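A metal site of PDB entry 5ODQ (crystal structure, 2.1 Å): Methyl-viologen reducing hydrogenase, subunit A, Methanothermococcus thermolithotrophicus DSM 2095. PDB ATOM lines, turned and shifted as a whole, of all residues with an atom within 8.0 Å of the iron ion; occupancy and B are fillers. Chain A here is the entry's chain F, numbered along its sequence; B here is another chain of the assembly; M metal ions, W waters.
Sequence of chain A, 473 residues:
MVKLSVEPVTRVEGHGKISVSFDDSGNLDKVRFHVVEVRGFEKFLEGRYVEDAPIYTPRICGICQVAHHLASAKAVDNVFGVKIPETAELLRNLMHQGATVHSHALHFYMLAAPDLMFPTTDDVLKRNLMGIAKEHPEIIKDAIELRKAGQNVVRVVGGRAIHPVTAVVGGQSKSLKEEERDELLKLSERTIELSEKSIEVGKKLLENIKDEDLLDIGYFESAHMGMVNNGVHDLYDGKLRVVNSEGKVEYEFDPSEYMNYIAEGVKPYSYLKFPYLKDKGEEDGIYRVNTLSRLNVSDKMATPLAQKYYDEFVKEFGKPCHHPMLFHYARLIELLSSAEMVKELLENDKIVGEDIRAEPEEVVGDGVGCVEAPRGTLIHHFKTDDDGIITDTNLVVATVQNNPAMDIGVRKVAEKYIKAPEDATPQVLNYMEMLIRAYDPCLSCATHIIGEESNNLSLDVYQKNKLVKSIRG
Water W3 lies within hydrogen-bond range of the side-chain amide oxygen (OD1) of Asn 394, the side-chain carboxylate (OE2) of Glu 264 and the side-chain amino group (NZ) of Lys 273.
Water W1 bridges the side-chain carboxylate of Glu 42 and the side-chain amino group of Lys 273.
The iron ion is bound by water W3, water W1, the backbone carbonyl oxygen (O) of Leu 395, a ring nitrogen (NE2) of His 448, the side-chain carboxylate (OE2) of Glu 42 and water W2.
NZ of Lys 273 touches the iron ion, at 3.7 Å.
A ring nitrogen (ND1) of His 448 sits close to the backbone carbonyl oxygen (O) of Ala 446, 3.3 Å away.
The backbone carbonyl oxygen of Cys 445 sits at hydrogen-bond distance from a ring nitrogen (ND1) of His 448 (2.8 Å).
The backbone carbonyl oxygen (O) of Glu 42 sits at hydrogen-bond distance from the side-chain hydroxyl (OG1) of Thr 393 (2.8 Å).
NZ of Lys 273 lies within salt-bridge range of OE2 of Glu 264.
NZ of Lys 273 is in hydrogen-bond range of OG1 of Thr 111 of chain B, 3.5 Å away.
The side-chain amino group (NZ) of Lys 273 sits at hydrogen-bond distance from the backbone carbonyl oxygen (O) of Ala 107 of chain B (2.8 Å).
The side-chain hydroxyl (OG1) of Thr 114 of chain B sits at hydrogen-bond distance from the side-chain amino group (NZ) of Lys 273, at 2.9 Å.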
ATOM      1  N   GLU A  42      -7.201  15.165  20.106  1.00  0.00           N
ATOM      2  CA  GLU A  42      -6.211  14.327  20.773  1.00  0.00           C
ATOM      3  C   GLU A  42      -5.946  14.765  22.198  1.00  0.00           C
ATOM      4  O   GLU A  42      -5.810  13.908  23.078  1.00  0.00           O
ATOM      5  CB  GLU A  42      -4.916  14.271  19.940  1.00  0.00           C
ATOM      6  CG  GLU A  42      -5.113  13.440  18.676  1.00  0.00           C
ATOM      7  CD  GLU A  42      -4.164  13.737  17.530  1.00  0.00           C
ATOM      8  OE1 GLU A  42      -3.822  14.923  17.308  1.00  0.00           O
ATOM      9  OE2 GLU A  42      -3.836  12.780  16.791  1.00  0.00           O
ATOM     10  N   GLU A 264       4.595  11.493  11.152  1.00  0.00           N
ATOM     11  CA  GLU A 264       3.849  12.627  10.626  1.00  0.00           C
ATOM     12  C   GLU A 264       4.632  13.906  10.750  1.00  0.00           C
ATOM     13  O   GLU A 264       4.866  14.390  11.859  1.00  0.00           O
ATOM     14  CB  GLU A 264       2.513  12.753  11.366  1.00  0.00           C
ATOM     15  CG  GLU A 264       1.651  11.517  11.251  1.00  0.00           C
ATOM     16  CD  GLU A 264       0.363  11.593  12.054  1.00  0.00           C
ATOM     17  OE1 GLU A 264      -0.670  11.974  11.472  1.00  0.00           O
ATOM     18  OE2 GLU A 264       0.399  11.250  13.255  1.00  0.00           O
ATOM     19  N   LEU A 272      -2.624  20.627   8.389  1.00  0.00           N
ATOM     20  CA  LEU A 272      -2.654  19.217   8.071  1.00  0.00           C
ATOM     21  C   LEU A 272      -1.248  18.694   8.064  1.00  0.00           C
ATOM     22  O   LEU A 272      -0.376  19.294   7.435  1.00  0.00           O
ATOM     23  CB  LEU A 272      -3.312  18.992   6.709  1.00  0.00           C
ATOM     24  CG  LEU A 272      -3.819  17.578   6.435  1.00  0.00           C
ATOM     25  CD1 LEU A 272      -4.290  16.916   7.704  1.00  0.00           C
ATOM     26  CD2 LEU A 272      -4.955  17.580   5.424  1.00  0.00           C
ATOM     27  N   LYS A 273      -0.998  17.597   8.779  1.00  0.00           N
ATOM     28  CA  LYS A 273       0.336  17.009   8.844  1.00  0.00           C
ATOM     29  C   LYS A 273       0.691  16.301   7.537  1.00  0.00           C
ATOM     30  O   LYS A 273      -0.161  16.077   6.691  1.00  0.00           O
ATOM     31  CB  LYS A 273       0.459  16.083  10.062  1.00  0.00           C
ATOM     32  CG  LYS A 273       0.707  16.874  11.360  1.00  0.00           C
ATOM     33  CD  LYS A 273      -0.060  16.327  12.588  1.00  0.00           C
ATOM     34  CE  LYS A 273       0.711  15.244  13.296  1.00  0.00           C
ATOM     35  NZ  LYS A 273      -0.038  14.701  14.462  1.00  0.00           N
ATOM     36  N   ILE A 379      -6.520   4.971  12.594  1.00  0.00           N
ATOM     37  CA  ILE A 379      -5.950   4.428  13.813  1.00  0.00           C
ATOM     38  C   ILE A 379      -6.265   5.345  14.980  1.00  0.00           C
ATOM     39  O   ILE A 379      -5.941   6.525  14.931  1.00  0.00           O
ATOM     40  CB  ILE A 379      -4.420   4.228  13.657  1.00  0.00           C
ATOM     41  CG1 ILE A 379      -4.121   3.076  12.668  1.00  0.00           C
ATOM     42  CG2 ILE A 379      -3.773   3.924  15.027  1.00  0.00           C
ATOM     43  CD1 ILE A 379      -2.884   3.253  11.934  1.00  0.00           C
ATOM     44  N   THR A 393      -3.566  10.396  23.884  1.00  0.00           N
ATOM     45  CA  THR A 393      -4.182   9.792  22.685  1.00  0.00           C
ATOM     46  C   THR A 393      -3.457  10.202  21.432  1.00  0.00           C
ATOM     47  O   THR A 393      -2.748  11.206  21.403  1.00  0.00           O
ATOM     48  CB  THR A 393      -5.648  10.204  22.488  1.00  0.00           C
ATOM     49  OG1 THR A 393      -5.703  11.445  21.798  1.00  0.00           O
ATOM     50  CG2 THR A 393      -6.441  10.274  23.767  1.00  0.00           C
ATOM     51  N   ASN A 394      -3.650   9.421  20.382  1.00  0.00           N
ATOM     52  CA  ASN A 394      -3.064   9.691  19.079  1.00  0.00           C
ATOM     53  C   ASN A 394      -3.985   9.169  18.019  1.00  0.00           C
ATOM     54  O   ASN A 394      -4.427   8.019  18.089  1.00  0.00           O
ATOM     55  CB  ASN A 394      -1.684   9.060  18.937  1.00  0.00           C
ATOM     56  CG  ASN A 394      -1.022   9.448  17.647  1.00  0.00           C
ATOM     57  OD1 ASN A 394      -1.045  10.608  17.230  1.00  0.00           O
ATOM     58  ND2 ASN A 394      -0.430   8.483  16.959  1.00  0.00           N
ATOM     59  N   LEU A 395      -4.291  10.007  17.030  1.00  0.00           N
ATOM     60  CA  LEU A 395      -5.178   9.637  15.957  1.00  0.00           C
ATOM     61  C   LEU A 395      -4.508   9.896  14.628  1.00  0.00           C
ATOM     62  O   LEU A 395      -4.143  11.037  14.322  1.00  0.00           O
ATOM     63  CB  LEU A 395      -6.465  10.459  15.994  1.00  0.00           C
ATOM     64  CG  LEU A 395      -7.162  10.634  17.333  1.00  0.00           C
ATOM     65  CD1 LEU A 395      -8.228  11.681  17.237  1.00  0.00           C
ATOM     66  CD2 LEU A 395      -7.757   9.330  17.806  1.00  0.00           C
ATOM     67  N   VAL A 396      -4.354   8.842  13.826  1.00  0.00           N
ATOM     68  CA  VAL A 396      -3.783   8.939  12.503  1.00  0.00           C
ATOM     69  C   VAL A 396      -5.029   8.724  11.668  1.00  0.00           C
ATOM     70  O   VAL A 396      -5.475   7.593  11.498  1.00  0.00           O
ATOM     71  CB  VAL A 396      -2.690   7.886  12.245  1.00  0.00           C
ATOM     72  CG1 VAL A 396      -1.906   8.218  10.982  1.00  0.00           C
ATOM     73  CG2 VAL A 396      -1.744   7.788  13.455  1.00  0.00           C
ATOM     74  N   VAL A 397      -5.631   9.835  11.210  1.00  0.00           N
ATOM     75  CA  VAL A 397      -6.891   9.784  10.477  1.00  0.00           C
ATOM     76  C   VAL A 397      -6.782   9.886   8.978  1.00  0.00           C
ATOM     77  O   VAL A 397      -6.447  10.934   8.427  1.00  0.00           O
ATOM     78  CB  VAL A 397      -7.836  10.864  11.017  1.00  0.00           C
ATOM     79  CG1 VAL A 397      -9.241  10.684  10.437  1.00  0.00           C
ATOM     80  CG2 VAL A 397      -7.891  10.836  12.547  1.00  0.00           C
ATOM     81  N   VAL A 400      -5.163  12.542   6.264  1.00  0.00           N
ATOM     82  CA  VAL A 400      -3.870  13.165   6.560  1.00  0.00           C
ATOM     83  C   VAL A 400      -2.750  12.486   5.740  1.00  0.00           C
ATOM     84  O   VAL A 400      -1.811  13.147   5.321  1.00  0.00           O
ATOM     85  CB  VAL A 400      -3.548  13.159   8.083  1.00  0.00           C
ATOM     86  CG1 VAL A 400      -3.295  11.747   8.607  1.00  0.00           C
ATOM     87  CG2 VAL A 400      -2.345  14.059   8.383  1.00  0.00           C
ATOM     88  N   CYS A 445     -11.722  15.627   9.378  1.00  0.00           N
ATOM     89  CA  CYS A 445     -11.250  14.303   9.791  1.00  0.00           C
ATOM     90  C   CYS A 445      -9.733  14.263   9.877  1.00  0.00           C
ATOM     91  O   CYS A 445      -9.176  13.824  10.883  1.00  0.00           O
ATOM     92  CB  CYS A 445     -11.751  13.255   8.807  1.00  0.00           C
ATOM     93  SG  CYS A 445     -12.520  11.822   9.586  1.00  0.00           S
ATOM     94  N   ALA A 446      -9.072  14.726   8.823  1.00  0.00           N
ATOM     95  CA  ALA A 446      -7.614  14.746   8.696  1.00  0.00           C
ATOM     96  C   ALA A 446      -6.893  15.548   9.779  1.00  0.00           C
ATOM     97  O   ALA A 446      -5.776  15.195  10.146  1.00  0.00           O
ATOM     98  CB  ALA A 446      -7.247  15.297   7.337  1.00  0.00           C
ATOM     99  N   THR A 447      -7.518  16.614  10.285  1.00  0.00           N
ATOM    100  CA  THR A 447      -6.912  17.468  11.309  1.00  0.00           C
ATOM    101  C   THR A 447      -7.350  17.092  12.714  1.00  0.00           C
ATOM    102  O   THR A 447      -6.539  17.142  13.632  1.00  0.00           O
ATOM    103  CB  THR A 447      -7.275  18.922  11.037  1.00  0.00           C
ATOM    104  OG1 THR A 447      -8.693  19.036  10.868  1.00  0.00           O
ATOM    105  CG2 THR A 447      -6.551  19.469   9.832  1.00  0.00           C
ATOM    106  N   HIS A 448      -8.627  16.722  12.886  1.00  0.00           N
ATOM    107  CA  HIS A 448      -9.168  16.347  14.188  1.00  0.00           C
ATOM    108  C   HIS A 448      -8.664  17.288  15.306  1.00  0.00           C
ATOM    109  O   HIS A 448      -8.780  18.528  15.122  1.00  0.00           O
ATOM    110  CB  HIS A 448      -8.892  14.848  14.514  1.00  0.00           C
ATOM    111  CG  HIS A 448      -7.515  14.360  14.160  1.00  0.00           C
ATOM    112  ND1 HIS A 448      -7.217  13.967  12.867  1.00  0.00           N
ATOM    113  CD2 HIS A 448      -6.430  14.185  14.933  1.00  0.00           C
ATOM    114  CE1 HIS A 448      -5.948  13.585  12.889  1.00  0.00           C
ATOM    115  NE2 HIS A 448      -5.425  13.694  14.114  1.00  0.00           N
ATOM    116  N   LYS B 106      -0.063  19.192  21.462  1.00  0.00           N
ATOM    117  CA  LYS B 106      -0.324  17.754  21.369  1.00  0.00           C
ATOM    118  C   LYS B 106      -0.367  17.334  19.909  1.00  0.00           C
ATOM    119  O   LYS B 106       0.361  16.414  19.515  1.00  0.00           O
ATOM    120  CB  LYS B 106      -1.666  17.397  22.039  1.00  0.00           C
ATOM    121  CG  LYS B 106      -2.062  15.908  21.903  1.00  0.00           C
ATOM    122  CD  LYS B 106      -0.987  14.927  22.384  1.00  0.00           C
ATOM    123  CE  LYS B 106      -0.646  15.095  23.846  1.00  0.00           C
ATOM    124  NZ  LYS B 106       0.431  14.171  24.270  1.00  0.00           N
ATOM    125  N   ALA B 107      -1.206  17.990  19.119  1.00  0.00           N
ATOM    126  CA  ALA B 107      -1.381  17.697  17.696  1.00  0.00           C
ATOM    127  C   ALA B 107      -0.135  17.872  16.841  1.00  0.00           C
ATOM    128  O   ALA B 107       0.082  17.059  15.940  1.00  0.00           O
ATOM    129  CB  ALA B 107      -2.492  18.563  17.140  1.00  0.00           C
ATOM    130  N   TYR B 108       0.678  18.905  17.088  1.00  0.00           N
ATOM    131  CA  TYR B 108       1.855  19.139  16.252  1.00  0.00           C
ATOM    132  C   TYR B 108       3.203  18.882  16.910  1.00  0.00           C
ATOM    133  O   TYR B 108       4.214  19.168  16.280  1.00  0.00           O
ATOM    134  CB  TYR B 108       1.783  20.557  15.695  1.00  0.00           C
ATOM    135  CG  TYR B 108       0.475  20.771  14.981  1.00  0.00           C
ATOM    136  CD1 TYR B 108       0.216  20.155  13.766  1.00  0.00           C
ATOM    137  CD2 TYR B 108      -0.554  21.497  15.566  1.00  0.00           C
ATOM    138  CE1 TYR B 108      -1.008  20.299  13.132  1.00  0.00           C
ATOM    139  CE2 TYR B 108      -1.781  21.654  14.943  1.00  0.00           C
ATOM    140  CZ  TYR B 108      -2.000  21.051  13.716  1.00  0.00           C
ATOM    141  OH  TYR B 108      -3.218  21.203  13.092  1.00  0.00           O
ATOM    142  N   THR B 111       2.397  14.163  19.914  1.00  0.00           N
ATOM    143  CA  THR B 111       1.663  12.930  19.599  1.00  0.00           C
ATOM    144  C   THR B 111       2.719  11.923  19.195  1.00  0.00           C
ATOM    145  O   THR B 111       3.645  12.280  18.476  1.00  0.00           O
ATOM    146  CB  THR B 111       0.597  13.158  18.527  1.00  0.00           C
ATOM    147  OG1 THR B 111       0.895  14.345  17.786  1.00  0.00           O
ATOM    148  CG2 THR B 111      -0.805  13.233  19.118  1.00  0.00           C
ATOM    149  N   THR B 113       3.282   9.611  16.936  1.00  0.00           N
ATOM    150  CA  THR B 113       3.757   9.523  15.549  1.00  0.00           C
ATOM    151  C   THR B 113       4.351  10.818  15.005  1.00  0.00           C
ATOM    152  O   THR B 113       5.078  10.777  14.014  1.00  0.00           O
ATOM    153  CB  THR B 113       2.628   9.098  14.621  1.00  0.00           C
ATOM    154  OG1 THR B 113       1.420   9.686  15.080  1.00  0.00           O
ATOM    155  CG2 THR B 113       2.472   7.615  14.558  1.00  0.00           C
ATOM    156  N   THR B 114       4.051  11.956  15.622  1.00  0.00           N
ATOM    157  CA  THR B 114       4.552  13.254  15.155  1.00  0.00           C
ATOM    158  C   THR B 114       6.052  13.417  15.225  1.00  0.00           C
ATOM    159  O   THR B 114       6.664  13.198  16.271  1.00  0.00           O
ATOM    160  CB  THR B 114       3.895  14.378  15.919  1.00  0.00           C
ATOM    161  OG1 THR B 114       2.484  14.248  15.764  1.00  0.00           O
ATOM    162  CG2 THR B 114       4.359  15.752  15.459  1.00  0.00           C
HETATM  163 FE    FE M   1      -3.351  13.002  14.579  1.00  0.00          FE
HETATM  164  O   HOH W   1      -2.758  14.916  14.838  1.00  0.00           O
HETATM  165  O   HOH W   2      -2.862  13.325  12.323  1.00  0.00           O
HETATM  166  O   HOH W   3      -1.694  12.213  15.260  1.00  0.00           O
